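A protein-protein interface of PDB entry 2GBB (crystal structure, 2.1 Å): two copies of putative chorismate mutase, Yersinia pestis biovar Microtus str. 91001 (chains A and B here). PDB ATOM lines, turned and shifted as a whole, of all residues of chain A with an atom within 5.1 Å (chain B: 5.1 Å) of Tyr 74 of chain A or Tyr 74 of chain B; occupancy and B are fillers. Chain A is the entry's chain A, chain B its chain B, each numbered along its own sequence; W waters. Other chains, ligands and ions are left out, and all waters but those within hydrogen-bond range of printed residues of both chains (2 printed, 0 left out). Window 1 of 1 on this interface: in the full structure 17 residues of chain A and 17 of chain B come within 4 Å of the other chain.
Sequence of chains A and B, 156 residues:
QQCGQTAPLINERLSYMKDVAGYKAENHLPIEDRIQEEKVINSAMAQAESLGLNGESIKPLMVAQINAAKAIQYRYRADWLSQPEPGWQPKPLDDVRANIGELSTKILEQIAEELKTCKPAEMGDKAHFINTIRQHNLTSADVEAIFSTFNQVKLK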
ATOM      1  N   ILE A  31      10.358  23.499 -15.127  1.00  0.00           N
ATOM      2  CA  ILE A  31      11.576  24.112 -15.673  1.00  0.00           C
ATOM      3  C   ILE A  31      11.718  23.822 -17.162  1.00  0.00           C
ATOM      4  O   ILE A  31      12.074  24.736 -17.948  1.00  0.00           O
ATOM      5  CB  ILE A  31      12.829  23.639 -14.947  1.00  0.00           C
ATOM      6  CG1 ILE A  31      12.849  24.234 -13.518  1.00  0.00           C
ATOM      7  CG2 ILE A  31      14.127  23.980 -15.794  1.00  0.00           C
ATOM      8  CD1 ILE A  31      12.314  25.752 -13.460  1.00  0.00           C
ATOM      9  N   GLU A  32      11.413  22.566 -17.534  1.00  0.00           N
ATOM     10  CA  GLU A  32      11.548  22.125 -18.916  1.00  0.00           C
ATOM     11  C   GLU A  32      10.285  22.381 -19.726  1.00  0.00           C
ATOM     12  O   GLU A  32       9.183  21.969 -19.367  1.00  0.00           O
ATOM     13  CB  GLU A  32      11.899  20.641 -18.994  1.00  0.00           C
ATOM     14  CG  GLU A  32      12.268  20.193 -20.438  1.00  0.00           C
ATOM     15  CD  GLU A  32      12.749  18.745 -20.467  1.00  0.00           C
ATOM     16  OE1 GLU A  32      13.893  18.470 -19.986  1.00  0.00           O
ATOM     17  OE2 GLU A  32      11.992  17.892 -20.956  1.00  0.00           O
ATOM     18  N   ALA A  69      21.272  26.643 -18.640  1.00  0.00           N
ATOM     19  CA  ALA A  69      20.213  27.449 -18.155  1.00  0.00           C
ATOM     20  C   ALA A  69      19.219  26.626 -17.300  1.00  0.00           C
ATOM     21  O   ALA A  69      18.894  27.035 -16.193  1.00  0.00           O
ATOM     22  CB  ALA A  69      19.508  28.077 -19.345  1.00  0.00           C
ATOM     23  N   LYS A  70      18.745  25.481 -17.803  1.00  0.00           N
ATOM     24  CA  LYS A  70      17.903  24.609 -16.978  1.00  0.00           C
ATOM     25  C   LYS A  70      18.608  24.161 -15.700  1.00  0.00           C
ATOM     26  O   LYS A  70      17.998  24.159 -14.605  1.00  0.00           O
ATOM     27  CB  LYS A  70      17.373  23.420 -17.781  1.00  0.00           C
ATOM     28  CG  LYS A  70      16.435  23.839 -18.941  1.00  0.00           C
ATOM     29  CD  LYS A  70      15.694  22.581 -19.503  1.00  0.00           C
ATOM     30  CE  LYS A  70      16.621  21.547 -20.057  1.00  0.00           C
ATOM     31  NZ  LYS A  70      15.843  20.706 -20.959  1.00  0.00           N
ATOM     32  N   ALA A  71      19.891  23.804 -15.816  1.00  0.00           N
ATOM     33  CA  ALA A  71      20.641  23.370 -14.638  1.00  0.00           C
ATOM     34  C   ALA A  71      20.563  24.473 -13.547  1.00  0.00           C
ATOM     35  O   ALA A  71      20.265  24.223 -12.379  1.00  0.00           O
ATOM     36  CB  ALA A  71      22.104  23.012 -15.026  1.00  0.00           C
ATOM     37  N   ILE A  72      20.787  25.711 -13.950  1.00  0.00           N
ATOM     38  CA  ILE A  72      20.744  26.849 -13.042  1.00  0.00           C
ATOM     39  C   ILE A  72      19.376  27.000 -12.388  1.00  0.00           C
ATOM     40  O   ILE A  72      19.258  27.188 -11.145  1.00  0.00           O
ATOM     41  CB  ILE A  72      21.085  28.127 -13.809  1.00  0.00           C
ATOM     42  CG1 ILE A  72      22.592  28.158 -14.133  1.00  0.00           C
ATOM     43  CG2 ILE A  72      20.601  29.345 -13.018  1.00  0.00           C
ATOM     44  CD1 ILE A  72      23.020  29.345 -15.002  1.00  0.00           C
ATOM     45  N   GLN A  73      18.341  26.935 -13.239  1.00  0.00           N
ATOM     46  CA  GLN A  73      16.968  27.090 -12.806  1.00  0.00           C
ATOM     47  C   GLN A  73      16.567  25.989 -11.845  1.00  0.00           C
ATOM     48  O   GLN A  73      15.938  26.261 -10.843  1.00  0.00           O
ATOM     49  CB  GLN A  73      16.018  27.086 -13.992  1.00  0.00           C
ATOM     50  CG  GLN A  73      16.209  28.283 -14.968  1.00  0.00           C
ATOM     51  CD  GLN A  73      15.357  28.066 -16.204  1.00  0.00           C
ATOM     52  OE1 GLN A  73      14.096  27.973 -15.982  1.00  0.00           O
ATOM     53  NE2 GLN A  73      15.858  27.862 -17.337  1.00  0.00           N
ATOM     54  N   TYR A  74      16.917  24.751 -12.172  1.00  0.00           N
ATOM     55  CA  TYR A  74      16.591  23.628 -11.289  1.00  0.00           C
ATOM     56  C   TYR A  74      17.165  23.813  -9.867  1.00  0.00           C
ATOM     57  O   TYR A  74      16.485  23.579  -8.864  1.00  0.00           O
ATOM     58  CB  TYR A  74      17.199  22.353 -11.867  1.00  0.00           C
ATOM     59  CG  TYR A  74      16.325  21.628 -12.881  1.00  0.00           C
ATOM     60  CD1 TYR A  74      14.975  21.389 -12.623  1.00  0.00           C
ATOM     61  CD2 TYR A  74      16.867  21.232 -14.138  1.00  0.00           C
ATOM     62  CE1 TYR A  74      14.162  20.726 -13.560  1.00  0.00           C
ATOM     63  CE2 TYR A  74      16.084  20.580 -15.075  1.00  0.00           C
ATOM     64  CZ  TYR A  74      14.757  20.342 -14.788  1.00  0.00           C
ATOM     65  OH  TYR A  74      14.051  19.702 -15.742  1.00  0.00           O
ATOM     66  N   ARG A  75      18.425  24.254  -9.836  1.00  0.00           N
ATOM     67  CA  ARG A  75      19.167  24.511  -8.635  1.00  0.00           C
ATOM     68  C   ARG A  75      18.533  25.619  -7.819  1.00  0.00           C
ATOM     69  O   ARG A  75      18.404  25.463  -6.607  1.00  0.00           O
ATOM     70  CB  ARG A  75      20.628  24.778  -8.988  1.00  0.00           C
ATOM     71  CG  ARG A  75      21.343  23.471  -9.250  1.00  0.00           C
ATOM     72  CD  ARG A  75      22.831  23.598  -9.692  1.00  0.00           C
ATOM     73  NE  ARG A  75      23.264  22.285 -10.188  1.00  0.00           N
ATOM     74  CZ  ARG A  75      23.907  22.065 -11.335  1.00  0.00           C
ATOM     75  NH1 ARG A  75      24.237  23.096 -12.125  1.00  0.00           N
ATOM     76  NH2 ARG A  75      24.210  20.807 -11.709  1.00  0.00           N
ATOM     77  N   TYR A  76      18.060  26.696  -8.483  1.00  0.00           N
ATOM     78  CA  TYR A  76      17.313  27.720  -7.796  1.00  0.00           C
ATOM     79  C   TYR A  76      16.025  27.190  -7.243  1.00  0.00           C
ATOM     80  O   TYR A  76      15.659  27.534  -6.099  1.00  0.00           O
ATOM     81  CB  TYR A  76      17.050  28.967  -8.672  1.00  0.00           C
ATOM     82  CG  TYR A  76      18.231  29.969  -8.644  1.00  0.00           C
ATOM     83  CD1 TYR A  76      18.484  30.756  -7.497  1.00  0.00           C
ATOM     84  CD2 TYR A  76      19.101  30.062  -9.722  1.00  0.00           C
ATOM     85  CE1 TYR A  76      19.583  31.667  -7.457  1.00  0.00           C
ATOM     86  CE2 TYR A  76      20.148  30.984  -9.745  1.00  0.00           C
ATOM     87  CZ  TYR A  76      20.415  31.767  -8.582  1.00  0.00           C
ATOM     88  OH  TYR A  76      21.490  32.651  -8.597  1.00  0.00           O
ATOM     89  N   ARG A  77      15.299  26.382  -8.030  1.00  0.00           N
ATOM     90  CA  ARG A  77      13.994  25.870  -7.521  1.00  0.00           C
ATOM     91  C   ARG A  77      14.247  25.079  -6.207  1.00  0.00           C
ATOM     92  O   ARG A  77      13.538  25.235  -5.218  1.00  0.00           O
ATOM     93  CB  ARG A  77      13.293  24.946  -8.529  1.00  0.00           C
ATOM     94  CG  ARG A  77      12.595  25.541  -9.687  1.00  0.00           C
ATOM     95  CD  ARG A  77      11.417  26.457  -9.309  1.00  0.00           C
ATOM     96  NE  ARG A  77      10.092  25.862  -9.119  1.00  0.00           N
ATOM     97  CZ  ARG A  77       9.294  25.432 -10.085  1.00  0.00           C
ATOM     98  NH1 ARG A  77       9.701  25.448 -11.334  1.00  0.00           N
ATOM     99  NH2 ARG A  77       8.107  24.932  -9.800  1.00  0.00           N
ATOM    100  N   ALA A  78      15.278  24.249  -6.218  1.00  0.00           N
ATOM    101  CA  ALA A  78      15.630  23.419  -5.056  1.00  0.00           C
ATOM    102  C   ALA A  78      15.906  24.290  -3.816  1.00  0.00           C
ATOM    103  O   ALA A  78      15.277  24.125  -2.742  1.00  0.00           O
ATOM    104  CB  ALA A  78      16.824  22.536  -5.409  1.00  0.00           C
ATOM    105  N   LEU A  81      13.019  26.248  -1.912  1.00  0.00           N
ATOM    106  CA  LEU A  81      12.122  25.410  -1.101  1.00  0.00           C
ATOM    107  C   LEU A  81      12.426  25.489   0.399  1.00  0.00           C
ATOM    108  O   LEU A  81      11.495  25.518   1.260  1.00  0.00           O
ATOM    109  CB  LEU A  81      12.092  23.955  -1.588  1.00  0.00           C
ATOM    110  CG  LEU A  81      11.457  23.693  -2.975  1.00  0.00           C
ATOM    111  CD1 LEU A  81      11.796  22.297  -3.407  1.00  0.00           C
ATOM    112  CD2 LEU A  81       9.943  23.909  -3.039  1.00  0.00           C
ATOM    113  N   ILE B  31       8.883  17.832 -11.782  1.00  0.00           N
ATOM    114  CA  ILE B  31       9.198  17.351 -10.426  1.00  0.00           C
ATOM    115  C   ILE B  31       7.973  17.603  -9.575  1.00  0.00           C
ATOM    116  O   ILE B  31       7.519  16.734  -8.837  1.00  0.00           O
ATOM    117  CB  ILE B  31      10.440  18.079  -9.864  1.00  0.00           C
ATOM    118  CG1 ILE B  31      11.695  17.572 -10.594  1.00  0.00           C
ATOM    119  CG2 ILE B  31      10.489  18.043  -8.321  1.00  0.00           C
ATOM    120  CD1 ILE B  31      11.628  16.046 -10.885  1.00  0.00           C
ATOM    121  N   GLU B  32       7.406  18.785  -9.724  1.00  0.00           N
ATOM    122  CA  GLU B  32       6.298  19.106  -8.879  1.00  0.00           C
ATOM    123  C   GLU B  32       5.001  18.568  -9.488  1.00  0.00           C
ATOM    124  O   GLU B  32       4.679  18.875 -10.641  1.00  0.00           O
ATOM    125  CB  GLU B  32       6.205  20.610  -8.646  1.00  0.00           C
ATOM    126  CG  GLU B  32       5.001  20.986  -7.827  1.00  0.00           C
ATOM    127  CD  GLU B  32       4.906  22.454  -7.610  1.00  0.00           C
ATOM    128  OE1 GLU B  32       5.532  22.953  -6.646  1.00  0.00           O
ATOM    129  OE2 GLU B  32       4.205  23.103  -8.403  1.00  0.00           O
ATOM    130  N   LYS B  70      11.477  17.083  -3.119  1.00  0.00           N
ATOM    131  CA  LYS B  70      11.576  17.870  -4.397  1.00  0.00           C
ATOM    132  C   LYS B  70      12.947  18.535  -4.630  1.00  0.00           C
ATOM    133  O   LYS B  70      13.492  18.495  -5.756  1.00  0.00           O
ATOM    134  CB  LYS B  70      10.449  18.964  -4.438  1.00  0.00           C
ATOM    135  CG  LYS B  70       9.048  18.350  -4.620  1.00  0.00           C
ATOM    136  CD  LYS B  70       8.038  19.398  -5.088  1.00  0.00           C
ATOM    137  CE  LYS B  70       7.930  20.482  -3.995  1.00  0.00           C
ATOM    138  NZ  LYS B  70       6.817  21.397  -4.333  1.00  0.00           N
ATOM    139  N   ALA B  71      13.515  19.126  -3.577  1.00  0.00           N
ATOM    140  CA  ALA B  71      14.854  19.686  -3.654  1.00  0.00           C
ATOM    141  C   ALA B  71      15.906  18.612  -4.068  1.00  0.00           C
ATOM    142  O   ALA B  71      16.712  18.869  -4.960  1.00  0.00           O
ATOM    143  CB  ALA B  71      15.261  20.394  -2.293  1.00  0.00           C
ATOM    144  N   ILE B  72      15.842  17.413  -3.479  1.00  0.00           N
ATOM    145  CA  ILE B  72      16.701  16.295  -3.936  1.00  0.00           C
ATOM    146  C   ILE B  72      16.483  16.052  -5.450  1.00  0.00           C
ATOM    147  O   ILE B  72      17.475  16.032  -6.245  1.00  0.00           O
ATOM    148  CB  ILE B  72      16.427  14.983  -3.163  1.00  0.00           C
ATOM    149  CG1 ILE B  72      17.018  15.065  -1.756  1.00  0.00           C
ATOM    150  CG2 ILE B  72      17.119  13.761  -3.814  1.00  0.00           C
ATOM    151  CD1 ILE B  72      16.494  13.925  -0.797  1.00  0.00           C
ATOM    152  N   GLN B  73      15.198  15.905  -5.844  1.00  0.00           N
ATOM    153  CA  GLN B  73      14.866  15.616  -7.234  1.00  0.00           C
ATOM    154  C   GLN B  73      15.332  16.694  -8.202  1.00  0.00           C
ATOM    155  O   GLN B  73      15.804  16.349  -9.260  1.00  0.00           O
ATOM    156  CB  GLN B  73      13.361  15.446  -7.451  1.00  0.00           C
ATOM    157  CG  GLN B  73      12.774  14.197  -6.805  1.00  0.00           C
ATOM    158  CD  GLN B  73      11.315  14.251  -6.791  1.00  0.00           C
ATOM    159  OE1 GLN B  73      10.759  14.115  -7.952  1.00  0.00           O
ATOM    160  NE2 GLN B  73      10.650  14.449  -5.731  1.00  0.00           N
ATOM    161  N   TYR B  74      15.086  17.973  -7.883  1.00  0.00           N
ATOM    162  CA  TYR B  74      15.531  19.126  -8.724  1.00  0.00           C
ATOM    163  C   TYR B  74      17.027  19.131  -8.963  1.00  0.00           C
ATOM    164  O   TYR B  74      17.476  19.466 -10.062  1.00  0.00           O
ATOM    165  CB  TYR B  74      15.133  20.476  -8.088  1.00  0.00           C
ATOM    166  CG  TYR B  74      13.661  20.881  -8.231  1.00  0.00           C
ATOM    167  CD1 TYR B  74      13.040  20.882  -9.488  1.00  0.00           C
ATOM    168  CD2 TYR B  74      12.928  21.361  -7.117  1.00  0.00           C
ATOM    169  CE1 TYR B  74      11.717  21.304  -9.665  1.00  0.00           C
ATOM    170  CE2 TYR B  74      11.576  21.770  -7.267  1.00  0.00           C
ATOM    171  CZ  TYR B  74      10.992  21.738  -8.551  1.00  0.00           C
ATOM    172  OH  TYR B  74       9.694  22.166  -8.746  1.00  0.00           O
ATOM    173  N   ARG B  75      17.816  18.799  -7.930  1.00  0.00           N
ATOM    174  CA  ARG B  75      19.280  18.778  -8.064  1.00  0.00           C
ATOM    175  C   ARG B  75      19.796  17.588  -8.861  1.00  0.00           C
ATOM    176  O   ARG B  75      20.797  17.719  -9.580  1.00  0.00           O
ATOM    177  CB  ARG B  75      19.961  18.802  -6.675  1.00  0.00           C
ATOM    178  CG  ARG B  75      19.712  20.118  -5.917  1.00  0.00           C
ATOM    179  CD  ARG B  75      20.162  20.104  -4.427  1.00  0.00           C
ATOM    180  NE  ARG B  75      19.901  21.418  -3.879  1.00  0.00           N
ATOM    181  CZ  ARG B  75      19.257  21.661  -2.739  1.00  0.00           C
ATOM    182  NH1 ARG B  75      18.900  20.667  -1.924  1.00  0.00           N
ATOM    183  NH2 ARG B  75      19.088  22.926  -2.366  1.00  0.00           N
ATOM    184  N   TYR B  76      19.130  16.425  -8.763  1.00  0.00           N
ATOM    185  CA  TYR B  76      19.439  15.346  -9.720  1.00  0.00           C
ATOM    186  C   TYR B  76      19.129  15.780 -11.133  1.00  0.00           C
ATOM    187  O   TYR B  76      19.943  15.552 -12.000  1.00  0.00           O
ATOM    188  CB  TYR B  76      18.735  14.010  -9.435  1.00  0.00           C
ATOM    189  CG  TYR B  76      19.425  13.240  -8.367  1.00  0.00           C
ATOM    190  CD1 TYR B  76      20.704  12.740  -8.572  1.00  0.00           C
ATOM    191  CD2 TYR B  76      18.801  13.001  -7.135  1.00  0.00           C
ATOM    192  CE1 TYR B  76      21.345  12.031  -7.597  1.00  0.00           C
ATOM    193  CE2 TYR B  76      19.431  12.278  -6.136  1.00  0.00           C
ATOM    194  CZ  TYR B  76      20.685  11.782  -6.371  1.00  0.00           C
ATOM    195  OH  TYR B  76      21.359  11.093  -5.385  1.00  0.00           O
ATOM    196  N   ARG B  77      17.982  16.416 -11.373  1.00  0.00           N
ATOM    197  CA  ARG B  77      17.661  16.810 -12.766  1.00  0.00           C
ATOM    198  C   ARG B  77      18.722  17.767 -13.284  1.00  0.00           C
ATOM    199  O   ARG B  77      19.128  17.711 -14.454  1.00  0.00           O
ATOM    200  CB  ARG B  77      16.274  17.499 -12.921  1.00  0.00           C
ATOM    201  CG  ARG B  77      15.072  16.662 -12.576  1.00  0.00           C
ATOM    202  CD  ARG B  77      14.728  15.582 -13.615  1.00  0.00           C
ATOM    203  NE  ARG B  77      14.270  16.023 -14.944  1.00  0.00           N
ATOM    204  CZ  ARG B  77      13.009  16.232 -15.381  1.00  0.00           C
ATOM    205  NH1 ARG B  77      11.930  16.200 -14.586  1.00  0.00           N
ATOM    206  NH2 ARG B  77      12.821  16.533 -16.670  1.00  0.00           N
ATOM    207  N   ALA B  78      19.153  18.689 -12.427  1.00  0.00           N
ATOM    208  CA  ALA B  78      20.235  19.614 -12.841  1.00  0.00           C
ATOM    209  C   ALA B  78      21.513  18.885 -13.170  1.00  0.00           C
ATOM    210  O   ALA B  78      22.086  19.134 -14.223  1.00  0.00           O
ATOM    211  CB  ALA B  78      20.495  20.730 -11.755  1.00  0.00           C
ATOM    212  N   LEU B  81      21.834  16.735 -16.541  1.00  0.00           N
ATOM    213  CA  LEU B  81      21.951  17.431 -17.838  1.00  0.00           C
ATOM    214  C   LEU B  81      23.382  17.379 -18.396  1.00  0.00           C
ATOM    215  O   LEU B  81      23.579  17.132 -19.605  1.00  0.00           O
ATOM    216  CB  LEU B  81      21.456  18.871 -17.722  1.00  0.00           C
ATOM    217  CG  LEU B  81      19.986  18.965 -17.318  1.00  0.00           C
ATOM    218  CD1 LEU B  81      19.637  20.325 -16.910  1.00  0.00           C
ATOM    219  CD2 LEU B  81      19.089  18.514 -18.444  1.00  0.00           C
HETATM  220  O   HOH W   1      22.561  19.955  -8.646  1.00  0.00           O
HETATM  221  O   HOH W   2      20.388  23.679  -5.483  1.00  0.00           O
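The side-chain hydroxyl (OH) of Tyr 74 of chain B lies within hydrogen-bond range of the guanidinium group (NH2) of Arg 77 of chain A (3.4 Å). The guanidinium group (NH2) of Arg 77 of chain B is in salt-bridge range of the side-chain carboxylate (OE1) of Glu 32 of chain A, 3.99 Å away.
The side-chain amino group (NZ) of Lys 70 of chain A lies within salt-bridge range of the side-chain carboxylate (OE1) of Glu 32 of chain A (3.1 Å). The side-chain carboxylate of Glu 32 of chain B is in salt-bridge range of the side-chain amino group of Lys 70 of chain B (3.1 Å).
Among the printed residues, pairs that only touch across the chains: Tyr 74 of chain A with Tyr 74 of chain B (3.4 Å), Tyr 74 of chain A with Arg 77 of chain B (3.5 Å), Arg 75 of chain A with Ala 78 of chain B (3.5 Å), Ala 71 of chain A with Ala 78 of chain B (3.6 Å), Leu 81 of chain A with Ala 71 of chain B (3.6 Å), Ala 78 of chain A with Arg 75 of chain B (3.6 Å), Ala 71 of chain A with Leu 81 of chain B (3.7 Å), Tyr 74 of chain A with Ala 78 of chain B (3.7 Å), Ala 78 of chain A with Ala 71 of chain B (3.7 Å), Leu 81 of chain A with Lys 70 of chain B (3.7 Å), Ala 78 of chain A with Tyr 74 of chain B (3.8 Å), Leu 81 of chain A with Tyr 74 of chain B (3.9 Å) and Lys 70 of chain A with Leu 81 of chain B (3.9 Å).
Printed residues of chain B within 4 Å of Tyr 74 of chain A: Tyr 74 (3.4 Å), Arg 77 (3.5 Å) and Ala 78 (3.7 Å). Printed residues of chain B within 4 Å of Arg 75 of chain A: Ala 78 (3.5 Å). Of the printed residues of chain B, Ala 78 of chain A touches Ala 71, Tyr 74 and Arg 75. Of the printed residues of chain B, Leu 81 of chain A touches Lys 70, Ala 71 and Tyr 74. The nearest printed residue of chain B that does not touch Leu 81 of chain A is Glu 32 of chain B (5.8 Å).
Hydrophobic or aromatic side chains of chain B within 4 Å of the printed part of chain A: Ala 71, Tyr 74, Ala 78 and Leu 81. Among the printed residues, Asp or Glu carboxylates within 4 Å of a Lys or Arg side-chain nitrogen of the other chain: Glu 32 of chain A with Arg 77 of chain B (3.99 Å).
Ala 71 of chain A touches Leu 81 of chain B, and with the chains exchanged Leu 81 of chain A touches Ala 71 of chain B. Tyr 74 of chain A touches its own counterpart, Tyr 74 of chain B. Tyr 74 of chain A touches Ala 78 of chain B, and with the chains exchanged Ala 78 of chain A touches Tyr 74 of chain B. Arg 75 of chain A touches Ala 78 of chain B, and with the chains exchanged Ala 78 of chain A touches Arg 75 of chain B. Positions printed for both chains: 31, 32, 70, 71, 72, 73, 74, 75, 76, 77, 78 and 81.
Water W2 lies within hydrogen-bond range of the guanidinium group (NE) of Arg 75 of chain B (2.8 Å) and the backbone carbonyl oxygen (O) of Arg 75 of chain A (2.9 Å). Water W1 lies within hydrogen-bond range of the guanidinium group of Arg 75 of chain A and the backbone carbonyl oxygen of Arg 75 of chain B.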
